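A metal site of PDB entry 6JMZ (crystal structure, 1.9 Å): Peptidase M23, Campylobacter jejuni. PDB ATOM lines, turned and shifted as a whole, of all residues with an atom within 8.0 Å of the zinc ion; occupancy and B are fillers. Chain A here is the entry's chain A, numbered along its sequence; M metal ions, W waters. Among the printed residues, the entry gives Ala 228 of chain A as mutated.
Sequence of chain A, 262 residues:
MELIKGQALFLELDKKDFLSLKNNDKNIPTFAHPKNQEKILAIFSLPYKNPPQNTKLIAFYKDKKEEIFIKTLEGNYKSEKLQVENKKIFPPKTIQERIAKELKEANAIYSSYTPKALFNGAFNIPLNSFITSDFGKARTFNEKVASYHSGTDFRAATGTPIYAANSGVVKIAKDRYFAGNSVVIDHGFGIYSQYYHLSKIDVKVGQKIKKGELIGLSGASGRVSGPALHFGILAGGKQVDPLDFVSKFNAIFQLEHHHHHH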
ATOM      1  N   THR A 132      -7.819  14.307  -3.783  1.00  0.00           N
ATOM      2  CA  THR A 132      -7.751  12.854  -3.768  1.00  0.00           C
ATOM      3  C   THR A 132      -8.720  12.204  -2.792  1.00  0.00           C
ATOM      4  O   THR A 132      -9.000  11.017  -2.916  1.00  0.00           O
ATOM      5  CB  THR A 132      -6.326  12.385  -3.410  1.00  0.00           C
ATOM      6  OG1 THR A 132      -5.946  12.953  -2.165  1.00  0.00           O
ATOM      7  CG2 THR A 132      -5.350  12.813  -4.474  1.00  0.00           C
ATOM      8  N   SER A 133      -9.237  12.961  -1.822  1.00  0.00           N
ATOM      9  CA  SER A 133     -10.254  12.440  -0.922  1.00  0.00           C
ATOM     10  C   SER A 133     -11.177  13.592  -0.574  1.00  0.00           C
ATOM     11  O   SER A 133     -10.754  14.560   0.065  1.00  0.00           O
ATOM     12  CB  SER A 133      -9.620  11.835   0.335  1.00  0.00           C
ATOM     13  OG  SER A 133     -10.601  11.246   1.152  1.00  0.00           O
ATOM     14  N   ASP A 134     -12.436  13.499  -0.991  1.00  0.00           N
ATOM     15  CA  ASP A 134     -13.347  14.631  -0.845  1.00  0.00           C
ATOM     16  C   ASP A 134     -13.875  14.745   0.585  1.00  0.00           C
ATOM     17  O   ASP A 134     -13.858  13.788   1.362  1.00  0.00           O
ATOM     18  CB  ASP A 134     -14.522  14.504  -1.819  1.00  0.00           C
ATOM     19  CG  ASP A 134     -15.037  15.859  -2.304  1.00  0.00           C
ATOM     20  OD1 ASP A 134     -16.076  15.881  -3.008  1.00  0.00           O
ATOM     21  OD2 ASP A 134     -14.413  16.901  -1.975  1.00  0.00           O
ATOM     22  N   PHE A 135     -14.373  15.939   0.900  1.00  0.00           N
ATOM     23  CA  PHE A 135     -15.061  16.193   2.163  1.00  0.00           C
ATOM     24  C   PHE A 135     -16.319  15.352   2.274  1.00  0.00           C
ATOM     25  O   PHE A 135     -17.025  15.126   1.294  1.00  0.00           O
ATOM     26  CB  PHE A 135     -15.418  17.671   2.256  1.00  0.00           C
ATOM     27  CG  PHE A 135     -16.312  18.026   3.439  1.00  0.00           C
ATOM     28  CD1 PHE A 135     -17.699  17.976   3.325  1.00  0.00           C
ATOM     29  CD2 PHE A 135     -15.748  18.447   4.633  1.00  0.00           C
ATOM     30  CE1 PHE A 135     -18.498  18.311   4.408  1.00  0.00           C
ATOM     31  CE2 PHE A 135     -16.547  18.782   5.716  1.00  0.00           C
ATOM     32  CZ  PHE A 135     -17.917  18.715   5.597  1.00  0.00           C
ATOM     33  N   TYR A 148     -16.656  10.860   9.639  1.00  0.00           N
ATOM     34  CA  TYR A 148     -16.676  11.432   8.309  1.00  0.00           C
ATOM     35  C   TYR A 148     -15.396  12.239   8.111  1.00  0.00           C
ATOM     36  O   TYR A 148     -14.721  12.627   9.065  1.00  0.00           O
ATOM     37  CB  TYR A 148     -17.931  12.298   8.094  1.00  0.00           C
ATOM     38  CG  TYR A 148     -17.872  13.649   8.764  1.00  0.00           C
ATOM     39  CD1 TYR A 148     -18.030  13.785  10.144  1.00  0.00           C
ATOM     40  CD2 TYR A 148     -17.657  14.803   8.016  1.00  0.00           C
ATOM     41  CE1 TYR A 148     -17.969  15.046  10.766  1.00  0.00           C
ATOM     42  CE2 TYR A 148     -17.589  16.049   8.633  1.00  0.00           C
ATOM     43  CZ  TYR A 148     -17.742  16.161   9.990  1.00  0.00           C
ATOM     44  OH  TYR A 148     -17.683  17.415  10.571  1.00  0.00           O
ATOM     45  N   HIS A 149     -15.054  12.462   6.846  1.00  0.00           N
ATOM     46  CA  HIS A 149     -13.873  13.246   6.492  1.00  0.00           C
ATOM     47  C   HIS A 149     -14.227  14.732   6.626  1.00  0.00           C
ATOM     48  O   HIS A 149     -15.063  15.240   5.867  1.00  0.00           O
ATOM     49  CB  HIS A 149     -13.439  12.904   5.066  1.00  0.00           C
ATOM     50  CG  HIS A 149     -12.101  13.445   4.685  1.00  0.00           C
ATOM     51  ND1 HIS A 149     -11.754  13.704   3.380  1.00  0.00           N
ATOM     52  CD2 HIS A 149     -11.016  13.764   5.438  1.00  0.00           C
ATOM     53  CE1 HIS A 149     -10.516  14.165   3.334  1.00  0.00           C
ATOM     54  NE2 HIS A 149     -10.045  14.197   4.572  1.00  0.00           N
ATOM     55  N   SER A 150     -13.596  15.424   7.567  1.00  0.00           N
ATOM     56  CA  SER A 150     -13.979  16.792   7.913  1.00  0.00           C
ATOM     57  C   SER A 150     -13.243  17.852   7.095  1.00  0.00           C
ATOM     58  O   SER A 150     -13.385  19.047   7.383  1.00  0.00           O
ATOM     59  CB  SER A 150     -13.747  17.041   9.398  1.00  0.00           C
ATOM     60  OG  SER A 150     -12.361  16.904   9.707  1.00  0.00           O
ATOM     61  N   GLY A 151     -12.433  17.462   6.114  1.00  0.00           N
ATOM     62  CA  GLY A 151     -11.832  18.414   5.206  1.00  0.00           C
ATOM     63  C   GLY A 151     -11.668  17.771   3.847  1.00  0.00           C
ATOM     64  O   GLY A 151     -12.333  16.776   3.555  1.00  0.00           O
ATOM     65  N   THR A 152     -10.789  18.308   2.998  1.00  0.00           N
ATOM     66  CA  THR A 152     -10.534  17.710   1.697  1.00  0.00           C
ATOM     67  C   THR A 152      -9.034  17.531   1.516  1.00  0.00           C
ATOM     68  O   THR A 152      -8.260  18.387   1.959  1.00  0.00           O
ATOM     69  CB  THR A 152     -11.167  18.571   0.578  1.00  0.00           C
ATOM     70  OG1 THR A 152     -11.082  17.877  -0.683  1.00  0.00           O
ATOM     71  CG2 THR A 152     -10.470  19.934   0.477  1.00  0.00           C
ATOM     72  N   ASP A 153      -8.618  16.424   0.905  1.00  0.00           N
ATOM     73  CA  ASP A 153      -7.192  16.123   0.744  1.00  0.00           C
ATOM     74  C   ASP A 153      -6.755  16.436  -0.672  1.00  0.00           C
ATOM     75  O   ASP A 153      -7.381  15.984  -1.624  1.00  0.00           O
ATOM     76  CB  ASP A 153      -6.897  14.651   1.041  1.00  0.00           C
ATOM     77  CG  ASP A 153      -7.202  14.280   2.480  1.00  0.00           C
ATOM     78  OD1 ASP A 153      -7.282  15.208   3.291  1.00  0.00           O
ATOM     79  OD2 ASP A 153      -7.364  13.083   2.779  1.00  0.00           O
ATOM     80  N   PHE A 154      -5.673  17.206  -0.788  1.00  0.00           N
ATOM     81  CA  PHE A 154      -5.021  17.506  -2.055  1.00  0.00           C
ATOM     82  C   PHE A 154      -3.839  16.578  -2.258  1.00  0.00           C
ATOM     83  O   PHE A 154      -3.084  16.318  -1.315  1.00  0.00           O
ATOM     84  CB  PHE A 154      -4.484  18.934  -2.080  1.00  0.00           C
ATOM     85  CG  PHE A 154      -5.527  19.990  -2.239  1.00  0.00           C
ATOM     86  CD1 PHE A 154      -6.251  20.451  -1.145  1.00  0.00           C
ATOM     87  CD2 PHE A 154      -5.761  20.555  -3.476  1.00  0.00           C
ATOM     88  CE1 PHE A 154      -7.193  21.451  -1.289  1.00  0.00           C
ATOM     89  CE2 PHE A 154      -6.701  21.569  -3.638  1.00  0.00           C
ATOM     90  CZ  PHE A 154      -7.417  22.019  -2.540  1.00  0.00           C
ATOM     91  N   TYR A 196      -3.209  20.605   7.412  1.00  0.00           N
ATOM     92  CA  TYR A 196      -2.752  19.538   8.291  1.00  0.00           C
ATOM     93  C   TYR A 196      -1.752  18.617   7.586  1.00  0.00           C
ATOM     94  O   TYR A 196      -1.665  18.573   6.349  1.00  0.00           O
ATOM     95  CB  TYR A 196      -3.952  18.693   8.795  1.00  0.00           C
ATOM     96  CG  TYR A 196      -4.922  19.434   9.700  1.00  0.00           C
ATOM     97  CD1 TYR A 196      -4.590  20.682  10.233  1.00  0.00           C
ATOM     98  CD2 TYR A 196      -6.159  18.893  10.026  1.00  0.00           C
ATOM     99  CE1 TYR A 196      -5.469  21.371  11.063  1.00  0.00           C
ATOM    100  CE2 TYR A 196      -7.049  19.575  10.861  1.00  0.00           C
ATOM    101  CZ  TYR A 196      -6.698  20.820  11.370  1.00  0.00           C
ATOM    102  OH  TYR A 196      -7.546  21.518  12.183  1.00  0.00           O
ATOM    103  N   HIS A 197      -0.988  17.888   8.421  1.00  0.00           N
ATOM    104  CA  HIS A 197      -0.030  16.872   8.018  1.00  0.00           C
ATOM    105  C   HIS A 197       1.237  17.443   7.389  1.00  0.00           C
ATOM    106  O   HIS A 197       1.923  16.748   6.637  1.00  0.00           O
ATOM    107  CB  HIS A 197      -0.676  15.836   7.081  1.00  0.00           C
ATOM    108  CG  HIS A 197      -1.985  15.327   7.588  1.00  0.00           C
ATOM    109  ND1 HIS A 197      -2.134  14.776   8.849  1.00  0.00           N
ATOM    110  CD2 HIS A 197      -3.222  15.310   7.034  1.00  0.00           C
ATOM    111  CE1 HIS A 197      -3.396  14.444   9.039  1.00  0.00           C
ATOM    112  NE2 HIS A 197      -4.081  14.759   7.953  1.00  0.00           N
ATOM    113  N   ARG A 223      -0.401  11.312   9.469  1.00  0.00           N
ATOM    114  CA  ARG A 223      -1.244  10.750   8.414  1.00  0.00           C
ATOM    115  C   ARG A 223      -0.875   9.300   8.173  1.00  0.00           C
ATOM    116  O   ARG A 223       0.310   8.956   8.091  1.00  0.00           O
ATOM    117  CB  ARG A 223      -1.126  11.562   7.125  1.00  0.00           C
ATOM    118  CG  ARG A 223      -2.261  11.332   6.138  1.00  0.00           C
ATOM    119  CD  ARG A 223      -2.347  12.433   5.093  1.00  0.00           C
ATOM    120  NE  ARG A 223      -3.567  12.319   4.294  1.00  0.00           N
ATOM    121  CZ  ARG A 223      -3.703  11.511   3.253  1.00  0.00           C
ATOM    122  NH1 ARG A 223      -2.688  10.739   2.865  1.00  0.00           N
ATOM    123  NH2 ARG A 223      -4.846  11.466   2.580  1.00  0.00           N
ATOM    124  N   SER A 225      -2.230   7.246   5.557  1.00  0.00           N
ATOM    125  CA  SER A 225      -2.256   6.841   4.154  1.00  0.00           C
ATOM    126  C   SER A 225      -1.268   7.631   3.289  1.00  0.00           C
ATOM    127  O   SER A 225      -1.535   7.855   2.101  1.00  0.00           O
ATOM    128  CB  SER A 225      -3.669   6.968   3.599  1.00  0.00           C
ATOM    129  OG  SER A 225      -4.300   8.142   4.081  1.00  0.00           O
ATOM    130  N   ALA A 228       0.005  13.906   1.868  1.00  0.00           N
ATOM    131  CA  ALA A 228      -1.081  14.686   1.255  1.00  0.00           C
ATOM    132  C   ALA A 228      -1.228  15.955   2.073  1.00  0.00           C
ATOM    133  O   ALA A 228      -0.694  16.069   3.177  1.00  0.00           O
ATOM    134  CB  ALA A 228      -2.417  13.932   1.236  1.00  0.00           C
ATOM    135  N   LEU A 229      -1.973  16.914   1.517  1.00  0.00           N
ATOM    136  CA  LEU A 229      -2.371  18.105   2.265  1.00  0.00           C
ATOM    137  C   LEU A 229      -3.852  17.989   2.612  1.00  0.00           C
ATOM    138  O   LEU A 229      -4.686  17.935   1.710  1.00  0.00           O
ATOM    139  CB  LEU A 229      -2.139  19.402   1.494  1.00  0.00           C
ATOM    140  CG  LEU A 229      -2.802  20.528   2.311  1.00  0.00           C
ATOM    141  CD1 LEU A 229      -1.873  20.948   3.454  1.00  0.00           C
ATOM    142  CD2 LEU A 229      -3.272  21.728   1.495  1.00  0.00           C
ATOM    143  N   HIS A 230      -4.171  17.989   3.905  1.00  0.00           N
ATOM    144  CA  HIS A 230      -5.556  18.047   4.349  1.00  0.00           C
ATOM    145  C   HIS A 230      -5.922  19.514   4.581  1.00  0.00           C
ATOM    146  O   HIS A 230      -5.275  20.194   5.383  1.00  0.00           O
ATOM    147  CB  HIS A 230      -5.758  17.219   5.622  1.00  0.00           C
ATOM    148  CG  HIS A 230      -7.075  17.445   6.302  1.00  0.00           C
ATOM    149  ND1 HIS A 230      -8.098  16.522   6.260  1.00  0.00           N
ATOM    150  CD2 HIS A 230      -7.533  18.484   7.038  1.00  0.00           C
ATOM    151  CE1 HIS A 230      -9.137  16.977   6.938  1.00  0.00           C
ATOM    152  NE2 HIS A 230      -8.817  18.169   7.420  1.00  0.00           N
ATOM    153  N   PHE A 231      -6.924  19.999   3.851  1.00  0.00           N
ATOM    154  CA  PHE A 231      -7.380  21.388   3.907  1.00  0.00           C
ATOM    155  C   PHE A 231      -8.788  21.415   4.489  1.00  0.00           C
ATOM    156  O   PHE A 231      -9.669  20.700   3.995  1.00  0.00           O
ATOM    157  CB  PHE A 231      -7.359  22.026   2.520  1.00  0.00           C
ATOM    158  CG  PHE A 231      -7.847  23.469   2.490  1.00  0.00           C
ATOM    159  CD1 PHE A 231      -7.164  24.458   3.179  1.00  0.00           C
ATOM    160  CD2 PHE A 231      -8.967  23.822   1.721  1.00  0.00           C
ATOM    161  CE1 PHE A 231      -7.603  25.787   3.140  1.00  0.00           C
ATOM    162  CE2 PHE A 231      -9.407  25.147   1.673  1.00  0.00           C
ATOM    163  CZ  PHE A 231      -8.725  26.127   2.389  1.00  0.00           C
ATOM    164  N   GLY A 232      -8.998  22.225   5.523  1.00  0.00           N
ATOM    165  CA  GLY A 232     -10.309  22.329   6.137  1.00  0.00           C
ATOM    166  C   GLY A 232     -10.732  23.773   6.298  1.00  0.00           C
ATOM    167  O   GLY A 232      -9.914  24.695   6.285  1.00  0.00           O
HETATM  168 ZN    ZN M   1      -8.149  14.730   5.139  1.00  0.00          ZN
HETATM  169  O   HOH W   1      -6.420  13.395   6.035  1.00  0.00           O
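Within 4 Å of the zinc ion: His 149, Asp 153 and His 230.
O of Gly 151 is in hydrogen-bond range of ND1 of His 149 (3.1 Å). The backbone carbonyl oxygen (O) of Asp 134 sits at hydrogen-bond distance from a ring nitrogen (ND1) of His 149 (2.9 Å). The guanidinium group of Arg 223 is in salt-bridge range of the side-chain carboxylate of Asp 153, at 3.0 Å. The backbone NH (N) of Asp 153 sits at hydrogen-bond distance from the backbone carbonyl oxygen (O) of Ser 133 (3.0 Å). The backbone carbonyl oxygen (O) of Asp 153 lies within hydrogen-bond range of the backbone NH (N) of Thr 132 (2.8 Å). The backbone carbonyl oxygen (O) of His 230 lies within hydrogen-bond range of the backbone NH (N) of Tyr 196 (2.9 Å).
Water W1 lies within hydrogen-bond range of a ring nitrogen (NE2) of His 197 (3.3 Å) and the side-chain carboxylate (OD2) of Asp 153 (3.4 Å).
A ring nitrogen (NE2) of His 149 binds the zinc ion, 2.0 Å away. The zinc ion is bound by OD1 of Asp 153 (2.1 Å). ND1 of His 230 binds the zinc ion, 2.1 Å away. Water W1 is bound to the zinc ion, 2.4 Å away.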
